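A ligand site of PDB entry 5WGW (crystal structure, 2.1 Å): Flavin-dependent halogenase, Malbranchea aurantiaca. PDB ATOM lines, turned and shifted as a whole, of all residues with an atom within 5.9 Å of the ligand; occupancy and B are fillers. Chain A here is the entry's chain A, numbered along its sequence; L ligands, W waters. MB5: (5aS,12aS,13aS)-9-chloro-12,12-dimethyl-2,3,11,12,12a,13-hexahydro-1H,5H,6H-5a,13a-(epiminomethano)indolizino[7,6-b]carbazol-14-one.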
ATOM      1  N   PRO A  85      15.405 -27.887  19.356  1.00  0.00           N
ATOM      2  CA  PRO A  85      13.985 -27.507  19.319  1.00  0.00           C
ATOM      3  C   PRO A  85      13.211 -27.990  18.105  1.00  0.00           C
ATOM      4  O   PRO A  85      12.011 -28.249  18.214  1.00  0.00           O
ATOM      5  CB  PRO A  85      14.050 -25.981  19.364  1.00  0.00           C
ATOM      6  CG  PRO A  85      15.261 -25.705  20.194  1.00  0.00           C
ATOM      7  CD  PRO A  85      16.254 -26.772  19.819  1.00  0.00           C
ATOM      8  N   GLY A 110      19.405 -25.524  26.469  1.00  0.00           N
ATOM      9  CA  GLY A 110      20.436 -24.721  25.831  1.00  0.00           C
ATOM     10  C   GLY A 110      21.761 -25.432  25.684  1.00  0.00           C
ATOM     11  O   GLY A 110      21.946 -26.613  25.994  1.00  0.00           O
ATOM     12  N   LEU A 111      22.728 -24.664  25.185  1.00  0.00           N
ATOM     13  CA  LEU A 111      24.077 -25.144  24.907  1.00  0.00           C
ATOM     14  C   LEU A 111      25.075 -24.262  25.629  1.00  0.00           C
ATOM     15  O   LEU A 111      24.927 -23.038  25.667  1.00  0.00           O
ATOM     16  CB  LEU A 111      24.372 -25.141  23.394  1.00  0.00           C
ATOM     17  CG  LEU A 111      23.636 -26.106  22.456  1.00  0.00           C
ATOM     18  CD1 LEU A 111      22.195 -25.708  22.227  1.00  0.00           C
ATOM     19  CD2 LEU A 111      24.376 -26.218  21.131  1.00  0.00           C
ATOM     20  N   SER A 129      24.142 -20.217  26.684  1.00  0.00           N
ATOM     21  CA  SER A 129      22.807 -19.822  26.259  1.00  0.00           C
ATOM     22  C   SER A 129      21.787 -20.641  27.026  1.00  0.00           C
ATOM     23  O   SER A 129      22.116 -21.666  27.638  1.00  0.00           O
ATOM     24  CB  SER A 129      22.610 -20.024  24.752  1.00  0.00           C
ATOM     25  OG  SER A 129      22.652 -21.398  24.422  1.00  0.00           O
ATOM     26  N   VAL A 130      20.553 -20.180  27.002  1.00  0.00           N
ATOM     27  CA  VAL A 130      19.458 -20.854  27.675  1.00  0.00           C
ATOM     28  C   VAL A 130      18.543 -21.481  26.622  1.00  0.00           C
ATOM     29  O   VAL A 130      18.651 -21.199  25.424  1.00  0.00           O
ATOM     30  CB  VAL A 130      18.670 -19.905  28.600  1.00  0.00           C
ATOM     31  CG1 VAL A 130      19.598 -19.348  29.686  1.00  0.00           C
ATOM     32  CG2 VAL A 130      18.053 -18.776  27.801  1.00  0.00           C
ATOM     33  N   GLY A 131      17.640 -22.340  27.082  1.00  0.00           N
ATOM     34  CA  GLY A 131      16.628 -22.914  26.219  1.00  0.00           C
ATOM     35  C   GLY A 131      15.368 -22.072  26.161  1.00  0.00           C
ATOM     36  O   GLY A 131      15.393 -20.956  25.647  1.00  0.00           O
ATOM     37  N   ALA A 132      14.274 -22.592  26.702  1.00  0.00           N
ATOM     38  CA  ALA A 132      12.979 -21.928  26.642  1.00  0.00           C
ATOM     39  C   ALA A 132      12.223 -22.205  27.933  1.00  0.00           C
ATOM     40  O   ALA A 132      12.526 -23.178  28.633  1.00  0.00           O
ATOM     41  CB  ALA A 132      12.153 -22.421  25.432  1.00  0.00           C
ATOM     42  N   PRO A 133      11.260 -21.354  28.297  1.00  0.00           N
ATOM     43  CA  PRO A 133      10.379 -21.679  29.420  1.00  0.00           C
ATOM     44  C   PRO A 133       9.625 -22.981  29.179  1.00  0.00           C
ATOM     45  O   PRO A 133       9.387 -23.399  28.039  1.00  0.00           O
ATOM     46  CB  PRO A 133       9.422 -20.479  29.494  1.00  0.00           C
ATOM     47  CG  PRO A 133      10.156 -19.362  28.847  1.00  0.00           C
ATOM     48  CD  PRO A 133      11.035 -19.989  27.784  1.00  0.00           C
ATOM     49  N   VAL A 136       6.865 -22.958  26.806  1.00  0.00           N
ATOM     50  CA  VAL A 136       7.208 -22.664  25.424  1.00  0.00           C
ATOM     51  C   VAL A 136       7.590 -23.962  24.720  1.00  0.00           C
ATOM     52  O   VAL A 136       6.838 -24.459  23.879  1.00  0.00           O
ATOM     53  CB  VAL A 136       8.333 -21.620  25.343  1.00  0.00           C
ATOM     54  CG1 VAL A 136       8.745 -21.371  23.900  1.00  0.00           C
ATOM     55  CG2 VAL A 136       7.874 -20.327  25.991  1.00  0.00           C
ATOM     56  N   LEU A 137       8.739 -24.529  25.062  1.00  0.00           N
ATOM     57  CA  LEU A 137       9.135 -25.842  24.545  1.00  0.00           C
ATOM     58  C   LEU A 137      10.239 -26.412  25.426  1.00  0.00           C
ATOM     59  O   LEU A 137      10.700 -25.792  26.385  1.00  0.00           O
ATOM     60  CB  LEU A 137       9.570 -25.750  23.076  1.00  0.00           C
ATOM     61  CG  LEU A 137      10.720 -24.841  22.632  1.00  0.00           C
ATOM     62  CD1 LEU A 137      12.100 -25.415  22.975  1.00  0.00           C
ATOM     63  CD2 LEU A 137      10.624 -24.571  21.136  1.00  0.00           C
ATOM     64  N   TYR A 408      27.013 -29.544  17.442  1.00  0.00           N
ATOM     65  CA  TYR A 408      25.729 -28.904  17.164  1.00  0.00           C
ATOM     66  C   TYR A 408      24.664 -29.908  16.718  1.00  0.00           C
ATOM     67  O   TYR A 408      23.576 -29.495  16.260  1.00  0.00           O
ATOM     68  CB  TYR A 408      25.847 -27.774  16.132  1.00  0.00           C
ATOM     69  CG  TYR A 408      26.457 -26.531  16.722  1.00  0.00           C
ATOM     70  CD1 TYR A 408      25.733 -25.740  17.602  1.00  0.00           C
ATOM     71  CD2 TYR A 408      27.765 -26.162  16.426  1.00  0.00           C
ATOM     72  CE1 TYR A 408      26.288 -24.607  18.164  1.00  0.00           C
ATOM     73  CE2 TYR A 408      28.333 -25.032  16.985  1.00  0.00           C
ATOM     74  CZ  TYR A 408      27.584 -24.250  17.853  1.00  0.00           C
ATOM     75  OH  TYR A 408      28.129 -23.128  18.418  1.00  0.00           O
ATOM     76  N   GLN A 488      26.959 -19.106  14.825  1.00  0.00           N
ATOM     77  CA  GLN A 488      26.096 -20.263  14.721  1.00  0.00           C
ATOM     78  C   GLN A 488      24.727 -19.978  15.337  1.00  0.00           C
ATOM     79  O   GLN A 488      23.704 -20.413  14.822  1.00  0.00           O
ATOM     80  CB  GLN A 488      26.729 -21.479  15.413  1.00  0.00           C
ATOM     81  CG  GLN A 488      26.217 -22.791  14.876  1.00  0.00           C
ATOM     82  CD  GLN A 488      26.734 -23.044  13.474  1.00  0.00           C
ATOM     83  OE1 GLN A 488      27.940 -23.109  13.246  1.00  0.00           O
ATOM     84  NE2 GLN A 488      25.813 -23.160  12.526  1.00  0.00           N
ATOM     85  N   PHE A 489      24.710 -19.231  16.441  1.00  0.00           N
ATOM     86  CA  PHE A 489      23.453 -18.898  17.103  1.00  0.00           C
ATOM     87  C   PHE A 489      22.674 -17.856  16.311  1.00  0.00           C
ATOM     88  O   PHE A 489      21.450 -17.964  16.182  1.00  0.00           O
ATOM     89  CB  PHE A 489      23.720 -18.425  18.533  1.00  0.00           C
ATOM     90  CG  PHE A 489      24.030 -19.547  19.499  1.00  0.00           C
ATOM     91  CD1 PHE A 489      25.112 -20.398  19.283  1.00  0.00           C
ATOM     92  CD2 PHE A 489      23.259 -19.736  20.637  1.00  0.00           C
ATOM     93  CE1 PHE A 489      25.402 -21.416  20.179  1.00  0.00           C
ATOM     94  CE2 PHE A 489      23.548 -20.754  21.532  1.00  0.00           C
ATOM     95  CZ  PHE A 489      24.620 -21.601  21.295  1.00  0.00           C
ATOM     96  N   GLY A 492      21.655 -19.608  12.925  1.00  0.00           N
ATOM     97  CA  GLY A 492      20.925 -20.848  13.069  1.00  0.00           C
ATOM     98  C   GLY A 492      19.750 -20.869  14.030  1.00  0.00           C
ATOM     99  O   GLY A 492      19.096 -21.910  14.137  1.00  0.00           O
ATOM    100  N   ILE A 493      19.466 -19.783  14.747  1.00  0.00           N
ATOM    101  CA  ILE A 493      18.298 -19.803  15.618  1.00  0.00           C
ATOM    102  C   ILE A 493      17.045 -19.931  14.753  1.00  0.00           C
ATOM    103  O   ILE A 493      16.964 -19.384  13.643  1.00  0.00           O
ATOM    104  CB  ILE A 493      18.274 -18.560  16.533  1.00  0.00           C
ATOM    105  CG1 ILE A 493      17.197 -18.724  17.595  1.00  0.00           C
ATOM    106  CG2 ILE A 493      18.081 -17.281  15.733  1.00  0.00           C
ATOM    107  CD1 ILE A 493      17.475 -17.929  18.842  1.00  0.00           C
ATOM    108  N   GLU A 494      16.067 -20.687  15.259  1.00  0.00           N
ATOM    109  CA  GLU A 494      14.944 -21.165  14.449  1.00  0.00           C
ATOM    110  C   GLU A 494      13.805 -20.143  14.471  1.00  0.00           C
ATOM    111  O   GLU A 494      12.802 -20.289  15.164  1.00  0.00           O
ATOM    112  CB  GLU A 494      14.479 -22.535  14.945  1.00  0.00           C
ATOM    113  CG  GLU A 494      15.587 -23.588  15.037  1.00  0.00           C
ATOM    114  CD  GLU A 494      16.185 -23.712  16.436  1.00  0.00           C
ATOM    115  OE1 GLU A 494      16.290 -22.690  17.153  1.00  0.00           O
ATOM    116  OE2 GLU A 494      16.540 -24.838  16.834  1.00  0.00           O
ATOM    117  N   ARG A 495      13.967 -19.090  13.662  1.00  0.00           N
ATOM    118  CA  ARG A 495      12.942 -18.061  13.569  1.00  0.00           C
ATOM    119  C   ARG A 495      11.631 -18.652  13.037  1.00  0.00           C
ATOM    120  O   ARG A 495      11.634 -19.474  12.119  1.00  0.00           O
ATOM    121  CB  ARG A 495      13.421 -16.920  12.672  1.00  0.00           C
ATOM    122  CG  ARG A 495      14.647 -16.187  13.183  1.00  0.00           C
ATOM    123  CD  ARG A 495      15.285 -15.309  12.103  1.00  0.00           C
ATOM    124  NE  ARG A 495      16.484 -14.631  12.601  1.00  0.00           N
ATOM    125  CZ  ARG A 495      17.670 -15.219  12.750  1.00  0.00           C
ATOM    126  NH1 ARG A 495      17.829 -16.491  12.431  1.00  0.00           N
ATOM    127  NH2 ARG A 495      18.700 -14.527  13.224  1.00  0.00           N
ATOM    128  N   LEU A 497       9.601 -20.794  14.306  1.00  0.00           N
ATOM    129  CA  LEU A 497       9.364 -22.208  14.553  1.00  0.00           C
ATOM    130  C   LEU A 497       7.953 -22.466  15.064  1.00  0.00           C
ATOM    131  O   LEU A 497       7.372 -23.527  14.790  1.00  0.00           O
ATOM    132  CB  LEU A 497      10.407 -22.739  15.542  1.00  0.00           C
ATOM    133  CG  LEU A 497      10.322 -24.184  16.041  1.00  0.00           C
ATOM    134  CD1 LEU A 497      10.445 -25.172  14.891  1.00  0.00           C
ATOM    135  CD2 LEU A 497      11.401 -24.430  17.093  1.00  0.00           C
ATOM    136  N   TRP A 514      20.960 -25.375  10.163  1.00  0.00           N
ATOM    137  CA  TRP A 514      21.683 -24.718  11.260  1.00  0.00           C
ATOM    138  C   TRP A 514      22.209 -23.338  10.864  1.00  0.00           C
ATOM    139  O   TRP A 514      23.153 -22.824  11.468  1.00  0.00           O
ATOM    140  CB  TRP A 514      22.842 -25.593  11.769  1.00  0.00           C
ATOM    141  CG  TRP A 514      22.627 -26.119  13.142  1.00  0.00           C
ATOM    142  CD1 TRP A 514      22.516 -27.434  13.505  1.00  0.00           C
ATOM    143  CD2 TRP A 514      22.493 -25.351  14.354  1.00  0.00           C
ATOM    144  NE1 TRP A 514      22.317 -27.534  14.868  1.00  0.00           N
ATOM    145  CE2 TRP A 514      22.295 -26.269  15.405  1.00  0.00           C
ATOM    146  CE3 TRP A 514      22.522 -23.983  14.637  1.00  0.00           C
ATOM    147  CZ2 TRP A 514      22.131 -25.862  16.730  1.00  0.00           C
ATOM    148  CZ3 TRP A 514      22.349 -23.580  15.952  1.00  0.00           C
ATOM    149  CH2 TRP A 514      22.159 -24.510  16.979  1.00  0.00           C
ATOM    150  N   LEU A 568      13.881 -10.387  19.160  1.00  0.00           N
ATOM    151  CA  LEU A 568      14.373 -11.416  20.056  1.00  0.00           C
ATOM    152  C   LEU A 568      15.139 -10.758  21.192  1.00  0.00           C
ATOM    153  O   LEU A 568      15.953  -9.866  20.951  1.00  0.00           O
ATOM    154  CB  LEU A 568      15.267 -12.406  19.298  1.00  0.00           C
ATOM    155  CG  LEU A 568      15.456 -13.789  19.925  1.00  0.00           C
ATOM    156  CD1 LEU A 568      14.212 -14.641  19.721  1.00  0.00           C
ATOM    157  CD2 LEU A 568      16.664 -14.468  19.336  1.00  0.00           C
ATOM    158  N   ILE A 573      18.919 -14.375  26.211  1.00  0.00           N
ATOM    159  CA  ILE A 573      19.220 -15.720  25.738  1.00  0.00           C
ATOM    160  C   ILE A 573      20.713 -16.021  25.807  1.00  0.00           C
ATOM    161  O   ILE A 573      21.114 -17.108  26.218  1.00  0.00           O
ATOM    162  CB  ILE A 573      18.686 -15.875  24.299  1.00  0.00           C
ATOM    163  CG1 ILE A 573      17.184 -15.584  24.273  1.00  0.00           C
ATOM    164  CG2 ILE A 573      18.968 -17.280  23.775  1.00  0.00           C
ATOM    165  CD1 ILE A 573      16.616 -15.547  22.888  1.00  0.00           C
ATOM    166  N   LEU A 574      21.562 -15.075  25.408  1.00  0.00           N
ATOM    167  CA  LEU A 574      23.010 -15.235  25.438  1.00  0.00           C
ATOM    168  C   LEU A 574      23.563 -14.493  26.641  1.00  0.00           C
ATOM    169  O   LEU A 574      23.424 -13.272  26.742  1.00  0.00           O
ATOM    170  CB  LEU A 574      23.652 -14.728  24.155  1.00  0.00           C
ATOM    171  CG  LEU A 574      23.176 -15.362  22.847  1.00  0.00           C
ATOM    172  CD1 LEU A 574      24.101 -14.946  21.708  1.00  0.00           C
ATOM    173  CD2 LEU A 574      23.112 -16.876  22.971  1.00  0.00           C
ATOM    174  N   TYR A 593      15.182 -20.722  33.430  1.00  0.00           N
ATOM    175  CA  TYR A 593      14.063 -21.564  33.039  1.00  0.00           C
ATOM    176  C   TYR A 593      14.010 -22.911  33.748  1.00  0.00           C
ATOM    177  O   TYR A 593      13.009 -23.622  33.612  1.00  0.00           O
ATOM    178  CB  TYR A 593      14.086 -21.822  31.521  1.00  0.00           C
ATOM    179  CG  TYR A 593      14.020 -20.605  30.638  1.00  0.00           C
ATOM    180  CD1 TYR A 593      13.249 -19.498  30.976  1.00  0.00           C
ATOM    181  CD2 TYR A 593      14.723 -20.562  29.437  1.00  0.00           C
ATOM    182  CE1 TYR A 593      13.186 -18.382  30.149  1.00  0.00           C
ATOM    183  CE2 TYR A 593      14.679 -19.462  28.608  1.00  0.00           C
ATOM    184  CZ  TYR A 593      13.907 -18.378  28.965  1.00  0.00           C
ATOM    185  OH  TYR A 593      13.874 -17.290  28.130  1.00  0.00           O
ATOM    186  N   LEU A 641       3.728 -14.561  25.185  1.00  0.00           N
ATOM    187  CA  LEU A 641       4.750 -15.528  24.784  1.00  0.00           C
ATOM    188  C   LEU A 641       4.201 -16.953  24.829  1.00  0.00           C
ATOM    189  O   LEU A 641       4.332 -17.709  23.853  1.00  0.00           O
ATOM    190  CB  LEU A 641       5.968 -15.390  25.690  1.00  0.00           C
ATOM    191  CG  LEU A 641       7.086 -16.429  25.561  1.00  0.00           C
ATOM    192  CD1 LEU A 641       7.596 -16.505  24.122  1.00  0.00           C
ATOM    193  CD2 LEU A 641       8.231 -16.105  26.510  1.00  0.00           C
ATOM    194  N   TRP A 645       3.006 -20.340  21.610  1.00  0.00           N
ATOM    195  CA  TRP A 645       3.566 -21.688  21.561  1.00  0.00           C
ATOM    196  C   TRP A 645       2.604 -22.755  22.044  1.00  0.00           C
ATOM    197  O   TRP A 645       2.999 -23.918  22.191  1.00  0.00           O
ATOM    198  CB  TRP A 645       4.860 -21.728  22.386  1.00  0.00           C
ATOM    199  CG  TRP A 645       5.934 -20.917  21.775  1.00  0.00           C
ATOM    200  CD1 TRP A 645       6.190 -19.590  21.974  1.00  0.00           C
ATOM    201  CD2 TRP A 645       6.909 -21.379  20.834  1.00  0.00           C
ATOM    202  NE1 TRP A 645       7.277 -19.190  21.226  1.00  0.00           N
ATOM    203  CE2 TRP A 645       7.738 -20.273  20.518  1.00  0.00           C
ATOM    204  CE3 TRP A 645       7.169 -22.607  20.233  1.00  0.00           C
ATOM    205  CZ2 TRP A 645       8.805 -20.372  19.617  1.00  0.00           C
ATOM    206  CZ3 TRP A 645       8.229 -22.707  19.339  1.00  0.00           C
ATOM    207  CH2 TRP A 645       9.034 -21.595  19.045  1.00  0.00           C
HETATM  208  N   MB5 L   1      13.719 -19.468  23.836  1.00  0.00           N
HETATM  209  C   MB5 L   1      12.433 -19.123  23.814  1.00  0.00           C
HETATM  210  O   MB5 L   1      11.738 -19.070  24.817  1.00  0.00           O
HETATM  211  C1  MB5 L   1      11.918 -18.827  22.403  1.00  0.00           C
HETATM  212  C10 MB5 L   1      20.168 -21.742  20.023  1.00  0.00           C
HETATM  213  C11 MB5 L   1      18.983 -21.990  19.363  1.00  0.00           C
HETATM  214  C12 MB5 L   1      17.801 -21.594  19.959  1.00  0.00           C
HETATM  215  C13 MB5 L   1      15.670 -21.132  20.479  1.00  0.00           C
HETATM  216  C14 MB5 L   1      14.165 -21.055  20.331  1.00  0.00           C
HETATM  217  C15 MB5 L   1      13.866 -20.114  19.155  1.00  0.00           C
HETATM  218  C16 MB5 L   1      13.657 -22.452  19.966  1.00  0.00           C
HETATM  219  C17 MB5 L   1      14.256 -18.103  21.955  1.00  0.00           C
HETATM  220  C18 MB5 L   1      12.341 -16.588  22.487  1.00  0.00           C
HETATM  221  C19 MB5 L   1      10.822 -16.673  22.361  1.00  0.00           C
HETATM  222  C2  MB5 L   1      12.093 -20.120  21.582  1.00  0.00           C
HETATM  223  C20 MB5 L   1      10.532 -18.165  22.371  1.00  0.00           C
HETATM  224  C3  MB5 L   1      13.565 -20.554  21.691  1.00  0.00           C
HETATM  225  C4  MB5 L   1      14.402 -19.517  22.534  1.00  0.00           C
HETATM  226  C5  MB5 L   1      15.840 -20.022  22.743  1.00  0.00           C
HETATM  227  C6  MB5 L   1      16.413 -20.664  21.524  1.00  0.00           C
HETATM  228  C7  MB5 L   1      17.790 -20.947  21.218  1.00  0.00           C
HETATM  229  C8  MB5 L   1      18.997 -20.714  21.853  1.00  0.00           C
HETATM  230  C9  MB5 L   1      20.189 -21.106  21.266  1.00  0.00           C
HETATM  231  N1  MB5 L   1      16.492 -21.701  19.533  1.00  0.00           N
HETATM  232  N2  MB5 L   1      12.821 -17.798  21.828  1.00  0.00           N
HETATM  233 CL   MB5 L   1      21.669 -22.223  19.289  1.00  0.00          CL
HETATM  234  O   HOH W   1      12.651 -13.233  22.912  1.00  0.00           O
HETATM  235  O   HOH W   2      19.247 -24.458  21.307  1.00  0.00           O
HETATM  236  O   HOH W   3      11.972 -16.659  26.492  1.00  0.00           O
HETATM  237  O   HOH W   4      11.278 -19.014  17.177  1.00  0.00           O
HETATM  238  O   HOH W   5      12.042 -17.188  19.225  1.00  0.00           O
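The backbone carbonyl oxygen (O) of Gly 131 lies within hydrogen-bond range of a nitrogen (N) of the ligand.
The side-chain carboxylate (OE1) of Glu 494 lies within hydrogen-bond range of a nitrogen (N1) of the ligand, at 2.6 Å.
The backbone carbonyl oxygen of Trp 514 sits at hydrogen-bond distance from the side-chain amide nitrogen of Gln 488, 2.9 Å away.
NE1 of Trp 514 sits at hydrogen-bond distance from O of Tyr 408 (2.7 Å).
The backbone carbonyl oxygen of Ile 573 sits at hydrogen-bond distance from the backbone NH of Val 130, 3.2 Å away.
The backbone carbonyl oxygen of Ile 493 is in hydrogen-bond range of the guanidinium group of Arg 495 (3.3 Å).
Residues that only touch the ligand: Pro 133 (3.2 Å), Phe 489 (3.2 Å), Trp 514 (3.3 Å), Ala 132 (3.4 Å), Trp 645 (3.6 Å), Pro 85 (3.6 Å), Ile 573 (3.6 Å), Val 130 (3.6 Å), Ile 493 (3.6 Å), Leu 641 (3.7 Å), Leu 568 (3.9 Å), Leu 137 (3.9 Å) and Val 136 (3.9 Å).
Within 4 Å of the ligand: Pro 85, Val 130, Gly 131, Ala 132, Pro 133, Val 136, Leu 137, Phe 489, Ile 493, Glu 494, Trp 514, Leu 568, Ile 573, Leu 641 and Trp 645.
The nearest printed residue that does not touch the ligand is Ser 129 (4.01 Å).
Water W3 lies within hydrogen-bond range of OH of Tyr 593 (2.6 Å) and O of the ligand (2.9 Å).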
